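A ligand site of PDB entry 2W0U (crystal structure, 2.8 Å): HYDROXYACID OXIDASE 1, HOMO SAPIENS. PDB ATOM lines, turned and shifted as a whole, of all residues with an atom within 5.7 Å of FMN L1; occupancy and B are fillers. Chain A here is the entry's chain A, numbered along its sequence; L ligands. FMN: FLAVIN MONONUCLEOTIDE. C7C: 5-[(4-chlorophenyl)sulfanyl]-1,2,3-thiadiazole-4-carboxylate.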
ATOM      1  N   TYR A  26       1.553   6.993  29.235  1.00  0.00           N
ATOM      2  CA  TYR A  26       0.746   8.184  29.485  1.00  0.00           C
ATOM      3  C   TYR A  26       1.309   9.425  28.760  1.00  0.00           C
ATOM      4  O   TYR A  26       0.541  10.201  28.171  1.00  0.00           O
ATOM      5  CB  TYR A  26       0.582   8.451  30.985  1.00  0.00           C
ATOM      6  CG  TYR A  26       0.255   9.899  31.256  1.00  0.00           C
ATOM      7  CD1 TYR A  26      -1.019  10.407  30.994  1.00  0.00           C
ATOM      8  CD2 TYR A  26       1.237  10.779  31.689  1.00  0.00           C
ATOM      9  CE1 TYR A  26      -1.308  11.741  31.200  1.00  0.00           C
ATOM     10  CE2 TYR A  26       0.952  12.106  31.899  1.00  0.00           C
ATOM     11  CZ  TYR A  26      -0.314  12.584  31.646  1.00  0.00           C
ATOM     12  OH  TYR A  26      -0.595  13.903  31.861  1.00  0.00           O
ATOM     13  N   TYR A  27       2.630   9.623  28.824  1.00  0.00           N
ATOM     14  CA  TYR A  27       3.286  10.775  28.188  1.00  0.00           C
ATOM     15  C   TYR A  27       3.332  10.675  26.660  1.00  0.00           C
ATOM     16  O   TYR A  27       3.278  11.687  25.969  1.00  0.00           O
ATOM     17  CB  TYR A  27       4.711  10.951  28.698  1.00  0.00           C
ATOM     18  CG  TYR A  27       4.876  11.463  30.125  1.00  0.00           C
ATOM     19  CD1 TYR A  27       4.236  12.612  30.557  1.00  0.00           C
ATOM     20  CD2 TYR A  27       5.727  10.801  31.023  1.00  0.00           C
ATOM     21  CE1 TYR A  27       4.402  13.084  31.839  1.00  0.00           C
ATOM     22  CE2 TYR A  27       5.902  11.271  32.316  1.00  0.00           C
ATOM     23  CZ  TYR A  27       5.237  12.410  32.712  1.00  0.00           C
ATOM     24  OH  TYR A  27       5.395  12.897  33.984  1.00  0.00           O
ATOM     25  N   SER A  29       1.254   8.704  24.532  1.00  0.00           N
ATOM     26  CA  SER A  29      -0.002   8.430  23.831  1.00  0.00           C
ATOM     27  C   SER A  29      -0.652   9.563  23.052  1.00  0.00           C
ATOM     28  O   SER A  29      -0.541  10.740  23.410  1.00  0.00           O
ATOM     29  CB  SER A  29      -1.038   7.878  24.802  1.00  0.00           C
ATOM     30  OG  SER A  29      -1.125   6.477  24.662  1.00  0.00           O
ATOM     31  N   ASN A  40       1.453  14.621  13.100  1.00  0.00           N
ATOM     32  CA  ASN A  40       2.142  15.794  13.641  1.00  0.00           C
ATOM     33  C   ASN A  40       3.598  15.792  13.224  1.00  0.00           C
ATOM     34  O   ASN A  40       4.139  16.838  12.883  1.00  0.00           O
ATOM     35  CB  ASN A  40       2.044  15.859  15.159  1.00  0.00           C
ATOM     36  CG  ASN A  40       0.792  16.585  15.661  1.00  0.00           C
ATOM     37  OD1 ASN A  40      -0.075  17.003  14.903  1.00  0.00           O
ATOM     38  ND2 ASN A  40       0.694  16.716  16.977  1.00  0.00           N
ATOM     39  N   GLY A  78       5.895  24.043  26.409  1.00  0.00           N
ATOM     40  CA  GLY A  78       4.442  23.901  26.461  1.00  0.00           C
ATOM     41  C   GLY A  78       3.976  23.272  27.751  1.00  0.00           C
ATOM     42  O   GLY A  78       4.759  22.692  28.490  1.00  0.00           O
ATOM     43  N   ALA A  79       2.676  23.391  28.020  1.00  0.00           N
ATOM     44  CA  ALA A  79       2.063  22.844  29.215  1.00  0.00           C
ATOM     45  C   ALA A  79       1.907  21.331  29.120  1.00  0.00           C
ATOM     46  O   ALA A  79       1.237  20.834  28.216  1.00  0.00           O
ATOM     47  CB  ALA A  79       0.728  23.468  29.425  1.00  0.00           C
ATOM     48  N   THR A  80       2.554  20.609  30.033  1.00  0.00           N
ATOM     49  CA  THR A  80       2.298  19.176  30.226  1.00  0.00           C
ATOM     50  C   THR A  80       2.067  18.896  31.704  1.00  0.00           C
ATOM     51  O   THR A  80       2.844  19.328  32.560  1.00  0.00           O
ATOM     52  CB  THR A  80       3.477  18.289  29.758  1.00  0.00           C
ATOM     53  OG1 THR A  80       4.589  18.477  30.645  1.00  0.00           O
ATOM     54  CG2 THR A  80       3.900  18.613  28.333  1.00  0.00           C
ATOM     55  N   ALA A  81       0.978  18.180  31.999  1.00  0.00           N
ATOM     56  CA  ALA A  81       0.579  17.891  33.376  1.00  0.00           C
ATOM     57  C   ALA A  81       1.499  16.885  34.048  1.00  0.00           C
ATOM     58  O   ALA A  81       2.135  16.070  33.370  1.00  0.00           O
ATOM     59  CB  ALA A  81      -0.847  17.382  33.402  1.00  0.00           C
ATOM     60  N   MET A 106       5.170  27.571  29.895  1.00  0.00           N
ATOM     61  CA  MET A 106       3.752  27.570  30.155  1.00  0.00           C
ATOM     62  C   MET A 106       3.542  26.549  31.273  1.00  0.00           C
ATOM     63  O   MET A 106       3.793  25.362  31.085  1.00  0.00           O
ATOM     64  CB  MET A 106       3.010  27.173  28.879  1.00  0.00           C
ATOM     65  CG  MET A 106       1.502  27.370  28.894  1.00  0.00           C
ATOM     66  SD  MET A 106       0.701  26.538  27.497  1.00  0.00           S
ATOM     67  CE  MET A 106       1.555  27.271  26.127  1.00  0.00           C
ATOM     68  N   SER A 108       1.417  24.158  33.386  1.00  0.00           N
ATOM     69  CA  SER A 108       0.239  23.393  33.053  1.00  0.00           C
ATOM     70  C   SER A 108      -0.764  23.385  34.191  1.00  0.00           C
ATOM     71  O   SER A 108      -0.429  23.608  35.352  1.00  0.00           O
ATOM     72  CB  SER A 108       0.631  21.971  32.686  1.00  0.00           C
ATOM     73  OG  SER A 108      -0.540  21.214  32.418  1.00  0.00           O
ATOM     74  N   SER A 109      -2.014  23.128  33.835  1.00  0.00           N
ATOM     75  CA  SER A 109      -3.014  22.767  34.811  1.00  0.00           C
ATOM     76  C   SER A 109      -2.676  21.348  35.282  1.00  0.00           C
ATOM     77  O   SER A 109      -2.024  20.594  34.565  1.00  0.00           O
ATOM     78  CB  SER A 109      -4.403  22.825  34.189  1.00  0.00           C
ATOM     79  OG  SER A 109      -4.475  21.989  33.051  1.00  0.00           O
ATOM     80  N   TRP A 110      -3.122  21.006  36.496  1.00  0.00           N
ATOM     81  CA  TRP A 110      -2.749  19.744  37.142  1.00  0.00           C
ATOM     82  C   TRP A 110      -1.230  19.572  37.217  1.00  0.00           C
ATOM     83  O   TRP A 110      -0.718  18.468  37.063  1.00  0.00           O
ATOM     84  CB  TRP A 110      -3.377  18.539  36.458  1.00  0.00           C
ATOM     85  CG  TRP A 110      -4.786  18.307  36.860  1.00  0.00           C
ATOM     86  CD1 TRP A 110      -5.219  17.749  38.031  1.00  0.00           C
ATOM     87  CD2 TRP A 110      -5.959  18.616  36.105  1.00  0.00           C
ATOM     88  NE1 TRP A 110      -6.599  17.698  38.041  1.00  0.00           N
ATOM     89  CE2 TRP A 110      -7.076  18.216  36.872  1.00  0.00           C
ATOM     90  CE3 TRP A 110      -6.179  19.196  34.840  1.00  0.00           C
ATOM     91  CZ2 TRP A 110      -8.377  18.368  36.424  1.00  0.00           C
ATOM     92  CZ3 TRP A 110      -7.471  19.347  34.403  1.00  0.00           C
ATOM     93  CH2 TRP A 110      -8.560  18.937  35.193  1.00  0.00           C
ATOM     94  N   GLN A 130      -1.233  28.057  31.877  1.00  0.00           N
ATOM     95  CA  GLN A 130      -2.283  27.375  31.141  1.00  0.00           C
ATOM     96  C   GLN A 130      -3.385  27.036  32.113  1.00  0.00           C
ATOM     97  O   GLN A 130      -3.137  26.621  33.246  1.00  0.00           O
ATOM     98  CB  GLN A 130      -1.763  26.114  30.434  1.00  0.00           C
ATOM     99  CG  GLN A 130      -2.800  25.415  29.540  1.00  0.00           C
ATOM    100  CD  GLN A 130      -3.600  24.357  30.279  1.00  0.00           C
ATOM    101  OE1 GLN A 130      -3.058  23.580  31.052  1.00  0.00           O
ATOM    102  NE2 GLN A 130      -4.897  24.334  30.060  1.00  0.00           N
ATOM    103  N   TYR A 132      -7.931  26.020  32.454  1.00  0.00           N
ATOM    104  CA  TYR A 132      -9.249  25.690  31.921  1.00  0.00           C
ATOM    105  C   TYR A 132     -10.265  26.551  32.620  1.00  0.00           C
ATOM    106  O   TYR A 132     -10.033  26.998  33.748  1.00  0.00           O
ATOM    107  CB  TYR A 132      -9.599  24.229  32.168  1.00  0.00           C
ATOM    108  CG  TYR A 132      -8.786  23.250  31.373  1.00  0.00           C
ATOM    109  CD1 TYR A 132      -8.998  23.094  30.012  1.00  0.00           C
ATOM    110  CD2 TYR A 132      -7.810  22.466  31.979  1.00  0.00           C
ATOM    111  CE1 TYR A 132      -8.263  22.185  29.288  1.00  0.00           C
ATOM    112  CE2 TYR A 132      -7.075  21.557  31.256  1.00  0.00           C
ATOM    113  CZ  TYR A 132      -7.304  21.427  29.909  1.00  0.00           C
ATOM    114  OH  TYR A 132      -6.569  20.532  29.187  1.00  0.00           O
ATOM    115  N   THR A 158      -7.080  26.751  27.406  1.00  0.00           N
ATOM    116  CA  THR A 158      -7.254  25.573  26.571  1.00  0.00           C
ATOM    117  C   THR A 158      -8.742  25.350  26.281  1.00  0.00           C
ATOM    118  O   THR A 158      -9.554  25.154  27.196  1.00  0.00           O
ATOM    119  CB  THR A 158      -6.595  24.342  27.210  1.00  0.00           C
ATOM    120  OG1 THR A 158      -5.193  24.602  27.364  1.00  0.00           O
ATOM    121  CG2 THR A 158      -6.752  23.123  26.359  1.00  0.00           C
ATOM    122  N   LYS A 236      -5.779  28.495  23.290  1.00  0.00           N
ATOM    123  CA  LYS A 236      -4.947  27.350  23.011  1.00  0.00           C
ATOM    124  C   LYS A 236      -5.788  26.166  22.497  1.00  0.00           C
ATOM    125  O   LYS A 236      -6.672  25.681  23.204  1.00  0.00           O
ATOM    126  CB  LYS A 236      -4.152  26.952  24.265  1.00  0.00           C
ATOM    127  CG  LYS A 236      -3.297  25.723  24.098  1.00  0.00           C
ATOM    128  CD  LYS A 236      -2.486  25.455  25.338  1.00  0.00           C
ATOM    129  CE  LYS A 236      -1.570  24.264  25.158  1.00  0.00           C
ATOM    130  NZ  LYS A 236      -2.314  22.985  24.983  1.00  0.00           N
ATOM    131  N   SER A 258      -2.974  24.270  18.037  1.00  0.00           N
ATOM    132  CA  SER A 258      -2.643  23.067  18.789  1.00  0.00           C
ATOM    133  C   SER A 258      -3.740  22.021  18.679  1.00  0.00           C
ATOM    134  O   SER A 258      -4.929  22.346  18.711  1.00  0.00           O
ATOM    135  CB  SER A 258      -2.424  23.425  20.256  1.00  0.00           C
ATOM    136  OG  SER A 258      -2.068  22.278  21.014  1.00  0.00           O
ATOM    137  N   ASN A 259      -3.341  20.760  18.518  1.00  0.00           N
ATOM    138  CA  ASN A 259      -4.284  19.651  18.588  1.00  0.00           C
ATOM    139  C   ASN A 259      -4.071  18.840  19.884  1.00  0.00           C
ATOM    140  O   ASN A 259      -4.393  17.646  19.976  1.00  0.00           O
ATOM    141  CB  ASN A 259      -4.277  18.795  17.315  1.00  0.00           C
ATOM    142  CG  ASN A 259      -2.925  18.185  16.989  1.00  0.00           C
ATOM    143  OD1 ASN A 259      -2.133  17.879  17.882  1.00  0.00           O
ATOM    144  ND2 ASN A 259      -2.652  17.986  15.706  1.00  0.00           N
ATOM    145  N   HIS A 260      -3.525  19.539  20.880  1.00  0.00           N
ATOM    146  CA  HIS A 260      -3.371  19.020  22.233  1.00  0.00           C
ATOM    147  C   HIS A 260      -2.423  17.821  22.239  1.00  0.00           C
ATOM    148  O   HIS A 260      -2.659  16.854  22.957  1.00  0.00           O
ATOM    149  CB  HIS A 260      -4.749  18.654  22.806  1.00  0.00           C
ATOM    150  CG  HIS A 260      -4.835  18.687  24.303  1.00  0.00           C
ATOM    151  ND1 HIS A 260      -5.663  19.552  24.974  1.00  0.00           N
ATOM    152  CD2 HIS A 260      -4.212  17.947  25.249  1.00  0.00           C
ATOM    153  CE1 HIS A 260      -5.547  19.359  26.278  1.00  0.00           C
ATOM    154  NE2 HIS A 260      -4.674  18.394  26.467  1.00  0.00           N
ATOM    155  N   GLY A 261      -1.365  17.877  21.431  1.00  0.00           N
ATOM    156  CA  GLY A 261      -0.437  16.759  21.295  1.00  0.00           C
ATOM    157  C   GLY A 261      -1.089  15.495  20.744  1.00  0.00           C
ATOM    158  O   GLY A 261      -0.690  14.384  21.076  1.00  0.00           O
ATOM    159  N   ARG A 263      -3.926  14.279  21.466  1.00  0.00           N
ATOM    160  CA  ARG A 263      -4.463  13.542  22.587  1.00  0.00           C
ATOM    161  C   ARG A 263      -5.992  13.675  22.722  1.00  0.00           C
ATOM    162  O   ARG A 263      -6.606  12.978  23.545  1.00  0.00           O
ATOM    163  CB  ARG A 263      -3.754  13.966  23.872  1.00  0.00           C
ATOM    164  CG  ARG A 263      -2.291  13.530  23.887  1.00  0.00           C
ATOM    165  CD  ARG A 263      -1.459  14.322  24.832  1.00  0.00           C
ATOM    166  NE  ARG A 263      -1.653  13.945  26.228  1.00  0.00           N
ATOM    167  CZ  ARG A 263      -0.991  12.978  26.869  1.00  0.00           C
ATOM    168  NH1 ARG A 263      -0.094  12.243  26.243  1.00  0.00           N
ATOM    169  NH2 ARG A 263      -1.242  12.743  28.149  1.00  0.00           N
ATOM    170  N   ASP A 291       2.192  24.283  18.397  1.00  0.00           N
ATOM    171  CA  ASP A 291       2.847  23.144  19.041  1.00  0.00           C
ATOM    172  C   ASP A 291       2.362  21.873  18.380  1.00  0.00           C
ATOM    173  O   ASP A 291       1.460  21.908  17.543  1.00  0.00           O
ATOM    174  CB  ASP A 291       2.589  23.118  20.548  1.00  0.00           C
ATOM    175  CG  ASP A 291       1.152  22.769  20.913  1.00  0.00           C
ATOM    176  OD1 ASP A 291       0.424  22.161  20.106  1.00  0.00           O
ATOM    177  OD2 ASP A 291       0.752  23.107  22.031  1.00  0.00           O
ATOM    178  N   GLY A 292       2.949  20.742  18.769  1.00  0.00           N
ATOM    179  CA  GLY A 292       2.566  19.453  18.199  1.00  0.00           C
ATOM    180  C   GLY A 292       3.537  19.014  17.119  1.00  0.00           C
ATOM    181  O   GLY A 292       3.492  19.538  16.029  1.00  0.00           O
ATOM    182  N   GLY A 293       4.421  18.083  17.452  1.00  0.00           N
ATOM    183  CA  GLY A 293       5.348  17.511  16.466  1.00  0.00           C
ATOM    184  C   GLY A 293       6.742  18.115  16.351  1.00  0.00           C
ATOM    185  O   GLY A 293       7.586  17.585  15.620  1.00  0.00           O
ATOM    186  N   VAL A 294       6.999  19.210  17.049  1.00  0.00           N
ATOM    187  CA  VAL A 294       8.295  19.882  16.960  1.00  0.00           C
ATOM    188  C   VAL A 294       9.360  19.060  17.654  1.00  0.00           C
ATOM    189  O   VAL A 294       9.301  18.841  18.861  1.00  0.00           O
ATOM    190  CB  VAL A 294       8.265  21.318  17.533  1.00  0.00           C
ATOM    191  CG1 VAL A 294       9.626  21.949  17.427  1.00  0.00           C
ATOM    192  CG2 VAL A 294       7.240  22.172  16.813  1.00  0.00           C
ATOM    193  N   ARG A 295      10.326  18.578  16.877  1.00  0.00           N
ATOM    194  CA  ARG A 295      11.388  17.713  17.387  1.00  0.00           C
ATOM    195  C   ARG A 295      12.757  18.129  16.861  1.00  0.00           C
ATOM    196  O   ARG A 295      13.785  17.691  17.373  1.00  0.00           O
ATOM    197  CB  ARG A 295      11.132  16.239  17.011  1.00  0.00           C
ATOM    198  CG  ARG A 295       9.732  15.703  17.337  1.00  0.00           C
ATOM    199  CD  ARG A 295       9.594  15.333  18.799  1.00  0.00           C
ATOM    200  NE  ARG A 295       8.297  14.736  19.106  1.00  0.00           N
ATOM    201  CZ  ARG A 295       7.262  15.412  19.615  1.00  0.00           C
ATOM    202  NH1 ARG A 295       7.361  16.710  19.848  1.00  0.00           N
ATOM    203  NH2 ARG A 295       6.120  14.792  19.880  1.00  0.00           N
ATOM    204  N   PHE A 312       5.900  25.782  20.671  1.00  0.00           N
ATOM    205  CA  PHE A 312       6.026  25.161  21.989  1.00  0.00           C
ATOM    206  C   PHE A 312       6.327  23.685  21.836  1.00  0.00           C
ATOM    207  O   PHE A 312       5.813  23.047  20.929  1.00  0.00           O
ATOM    208  CB  PHE A 312       4.746  25.370  22.826  1.00  0.00           C
ATOM    209  CG  PHE A 312       4.457  26.821  23.132  1.00  0.00           C
ATOM    210  CD1 PHE A 312       4.868  27.376  24.320  1.00  0.00           C
ATOM    211  CD2 PHE A 312       3.789  27.623  22.198  1.00  0.00           C
ATOM    212  CE1 PHE A 312       4.603  28.731  24.598  1.00  0.00           C
ATOM    213  CE2 PHE A 312       3.536  28.973  22.458  1.00  0.00           C
ATOM    214  CZ  PHE A 312       3.944  29.520  23.657  1.00  0.00           C
ATOM    215  N   VAL A 313       7.178  23.155  22.698  1.00  0.00           N
ATOM    216  CA  VAL A 313       7.433  21.722  22.731  1.00  0.00           C
ATOM    217  C   VAL A 313       6.820  21.096  23.986  1.00  0.00           C
ATOM    218  O   VAL A 313       6.901  21.669  25.070  1.00  0.00           O
ATOM    219  CB  VAL A 313       8.950  21.367  22.604  1.00  0.00           C
ATOM    220  CG1 VAL A 313       9.406  21.519  21.189  1.00  0.00           C
ATOM    221  CG2 VAL A 313       9.794  22.242  23.506  1.00  0.00           C
ATOM    222  N   GLY A 314       6.173  19.944  23.826  1.00  0.00           N
ATOM    223  CA  GLY A 314       5.582  19.214  24.941  1.00  0.00           C
ATOM    224  C   GLY A 314       6.434  18.031  25.355  1.00  0.00           C
ATOM    225  O   GLY A 314       7.311  18.150  26.210  1.00  0.00           O
ATOM    226  N   ARG A 315       6.186  16.885  24.733  1.00  0.00           N
ATOM    227  CA  ARG A 315       6.895  15.648  25.058  1.00  0.00           C
ATOM    228  C   ARG A 315       8.437  15.725  25.197  1.00  0.00           C
ATOM    229  O   ARG A 315       8.990  15.135  26.131  1.00  0.00           O
ATOM    230  CB  ARG A 315       6.481  14.533  24.095  1.00  0.00           C
ATOM    231  CG  ARG A 315       5.074  14.036  24.327  1.00  0.00           C
ATOM    232  CD  ARG A 315       4.704  12.915  23.358  1.00  0.00           C
ATOM    233  NE  ARG A 315       3.273  12.659  23.356  1.00  0.00           N
ATOM    234  CZ  ARG A 315       2.396  13.367  22.672  1.00  0.00           C
ATOM    235  NH1 ARG A 315       2.804  14.369  21.907  1.00  0.00           N
ATOM    236  NH2 ARG A 315       1.098  13.069  22.735  1.00  0.00           N
ATOM    237  N   PRO A 316       9.138  16.399  24.267  1.00  0.00           N
ATOM    238  CA  PRO A 316      10.586  16.508  24.433  1.00  0.00           C
ATOM    239  C   PRO A 316      11.070  17.001  25.788  1.00  0.00           C
ATOM    240  O   PRO A 316      12.135  16.591  26.235  1.00  0.00           O
ATOM    241  CB  PRO A 316      10.980  17.478  23.327  1.00  0.00           C
ATOM    242  CG  PRO A 316       9.978  17.246  22.277  1.00  0.00           C
ATOM    243  CD  PRO A 316       8.701  17.026  23.012  1.00  0.00           C
ATOM    244  N   VAL A 318       9.524  16.532  28.725  1.00  0.00           N
ATOM    245  CA  VAL A 318       9.300  15.383  29.596  1.00  0.00           C
ATOM    246  C   VAL A 318      10.387  14.333  29.434  1.00  0.00           C
ATOM    247  O   VAL A 318      10.845  13.771  30.429  1.00  0.00           O
ATOM    248  CB  VAL A 318       7.916  14.737  29.334  1.00  0.00           C
ATOM    249  CG1 VAL A 318       7.728  13.552  30.219  1.00  0.00           C
ATOM    250  CG2 VAL A 318       6.808  15.730  29.566  1.00  0.00           C
HETATM  251  N1  FMN L   1      -2.341  20.827  27.139  1.00  0.00           N
HETATM  252  C2  FMN L   1      -3.068  21.622  27.983  1.00  0.00           C
HETATM  253  O2  FMN L   1      -3.617  22.626  27.527  1.00  0.00           O
HETATM  254  N3  FMN L   1      -3.189  21.296  29.316  1.00  0.00           N
HETATM  255  C4  FMN L   1      -2.562  20.167  29.816  1.00  0.00           C
HETATM  256  O4  FMN L   1      -2.637  19.893  31.010  1.00  0.00           O
HETATM  257  C4A FMN L   1      -1.815  19.365  28.966  1.00  0.00           C
HETATM  258  N5  FMN L   1      -1.192  18.245  29.443  1.00  0.00           N
HETATM  259  C5A FMN L   1      -0.453  17.443  28.599  1.00  0.00           C
HETATM  260  C6  FMN L   1       0.182  16.300  29.091  1.00  0.00           C
HETATM  261  C7  FMN L   1       0.946  15.483  28.245  1.00  0.00           C
HETATM  262  C7M FMN L   1       1.890  14.487  28.832  1.00  0.00           C
HETATM  263  C8  FMN L   1       1.066  15.825  26.896  1.00  0.00           C
HETATM  264  C8M FMN L   1       1.973  15.037  25.996  1.00  0.00           C
HETATM  265  C9  FMN L   1       0.419  16.961  26.403  1.00  0.00           C
HETATM  266  C9A FMN L   1      -0.340  17.770  27.254  1.00  0.00           C
HETATM  267  N10 FMN L   1      -0.967  18.897  26.771  1.00  0.00           N
HETATM  268  C10 FMN L   1      -1.706  19.700  27.616  1.00  0.00           C
HETATM  269  C1' FMN L   1      -0.745  19.326  25.351  1.00  0.00           C
HETATM  270  C2' FMN L   1       0.493  20.196  25.273  1.00  0.00           C
HETATM  271  O2' FMN L   1       0.223  21.452  25.847  1.00  0.00           O
HETATM  272  C3' FMN L   1       0.933  20.421  23.842  1.00  0.00           C
HETATM  273  O3' FMN L   1      -0.199  20.800  23.101  1.00  0.00           O
HETATM  274  C4' FMN L   1       1.518  19.184  23.179  1.00  0.00           C
HETATM  275  O4' FMN L   1       2.291  18.455  24.098  1.00  0.00           O
HETATM  276  C5' FMN L   1       2.392  19.601  22.011  1.00  0.00           C
HETATM  277  O5' FMN L   1       2.744  18.448  21.286  1.00  0.00           O
HETATM  278  P   FMN L   1       4.179  17.744  21.474  1.00  0.00           P
HETATM  279  O1P FMN L   1       4.423  16.898  20.244  1.00  0.00           O
HETATM  280  O2P FMN L   1       4.160  16.900  22.730  1.00  0.00           O
HETATM  281  O3P FMN L   1       5.264  18.767  21.598  1.00  0.00           O
HETATM  282 CL   C7C L   2      -6.622  15.022  37.731  1.00  0.00          CL
HETATM  283  C1  C7C L   2      -5.865  14.951  36.105  1.00  0.00           C
HETATM  284  C2  C7C L   2      -4.481  15.036  35.983  1.00  0.00           C
HETATM  285  C3  C7C L   2      -3.898  14.978  34.724  1.00  0.00           C
HETATM  286  C6  C7C L   2      -6.655  14.815  34.969  1.00  0.00           C
HETATM  287  C5  C7C L   2      -6.067  14.764  33.717  1.00  0.00           C
HETATM  288  C4  C7C L   2      -4.687  14.843  33.588  1.00  0.00           C
HETATM  289  S8  C7C L   2      -3.964  14.775  32.055  1.00  0.00           S
HETATM  290  C9  C7C L   2      -4.442  16.182  31.135  1.00  0.00           C
HETATM  291  C13 C7C L   2      -4.108  16.406  29.709  1.00  0.00           C
HETATM  292  C14 C7C L   2      -3.304  15.408  28.953  1.00  0.00           C
HETATM  293  O15 C7C L   2      -2.650  14.556  29.578  1.00  0.00           O
HETATM  294  O16 C7C L   2      -3.313  15.454  27.697  1.00  0.00           O
HETATM  295  S10 C7C L   2      -5.358  17.503  31.736  1.00  0.00           S
HETATM  296  N11 C7C L   2      -5.353  18.342  30.264  1.00  0.00           N
HETATM  297  N12 C7C L   2      -4.626  17.605  29.288  1.00  0.00           N
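The side-chain hydroxyl (OG) of Ser 258 is in hydrogen-bond range of an oxygen (O3') of FMN L1, at 3.2 Å.
N11 of C7C L2 sits at hydrogen-bond distance from OH of Tyr 132.
N of Gly 292 sits close to O5' of FMN L1, at 3.4 Å.
NH1 of Arg 315 is in salt-bridge range of O2P of FMN L1, at 3.0 Å.
An oxygen (O2') of FMN L1 is in hydrogen-bond range of the backbone carbonyl oxygen (O) of Ala 79, at 2.6 Å.
The side-chain hydroxyl (OG) of Ser 108 is in hydrogen-bond range of an oxygen (O4) of FMN L1 (2.9 Å).
O2 of FMN L1 is in hydrogen-bond range of NZ of Lys 236.
NH2 of Arg 295 lies within salt-bridge range of O1P of FMN L1.
A nitrogen (N12) of C7C L2 is in hydrogen-bond range of a ring nitrogen (NE2) of His 260, at 2.9 Å.
OD2 of Asp 291 sits at hydrogen-bond distance from O3' of FMN L1 (2.7 Å).
O2 of FMN L1 sits at hydrogen-bond distance from OG1 of Thr 158, 2.5 Å away.
O4 of FMN L1 sits at hydrogen-bond distance from OG of Ser 109 (3.5 Å).
The backbone NH (N) of Gly 314 is in hydrogen-bond range of an oxygen (O3P) of FMN L1, 2.7 Å away.
The backbone NH of Ala 81 sits at hydrogen-bond distance from a nitrogen (N5) of FMN L1, at 3.4 Å.
O2P of FMN L1 sits at hydrogen-bond distance from N of Arg 315 (2.8 Å).
A nitrogen (N1) of FMN L1 is in hydrogen-bond range of a ring nitrogen (NE2) of His 260, at 3.4 Å.
The side-chain amide oxygen of Gln 130 lies within hydrogen-bond range of a nitrogen (N3) of FMN L1 (2.9 Å).
OH of Tyr 132 sits at hydrogen-bond distance from N3 of FMN L1 (3.5 Å).
O16 of C7C L2 is in salt-bridge range of NE of Arg 263.
OH of Tyr 26 lies within hydrogen-bond range of O15 of C7C L2 (3.1 Å).
The backbone NH (N) of Gly 293 lies within hydrogen-bond range of an oxygen (O1P) of FMN L1, at 3.0 Å.
Merely in contact with FMN L1: Arg 263 (3.4 Å), Tyr 27 (3.5 Å), Gly 261 (3.6 Å), Thr 80 (3.6 Å), Val 313 (3.7 Å) and Tyr 26 (3.7 Å).
Hydrophobic or aromatic side chains within 4 Å of FMN L1: Tyr 26, Tyr 27, Ala 81 and His 260.
The side-chain hydroxyl (OG) of Ser 108 sits at hydrogen-bond distance from the backbone NH (N) of Ala 81 (3.4 Å).
The guanidinium group of Arg 315 sits at hydrogen-bond distance from the backbone carbonyl oxygen of Ser 29 (2.9 Å).
OE1 of Gln 130 lies within hydrogen-bond range of OG of Ser 109 (2.9 Å).
O of Ser 29 is in hydrogen-bond range of NH1 of Arg 263, 3.2 Å away.
N of His 260 lies within hydrogen-bond range of OG of Ser 258 (3.1 Å).
O of Val 313 lies within hydrogen-bond range of N of Gly 78 (2.9 Å).
The side-chain amide nitrogen of Gln 130 lies within hydrogen-bond range of the side-chain hydroxyl of Thr 158.
The backbone carbonyl oxygen of Gly 261 sits at hydrogen-bond distance from the guanidinium group of Arg 315, at 2.8 Å.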
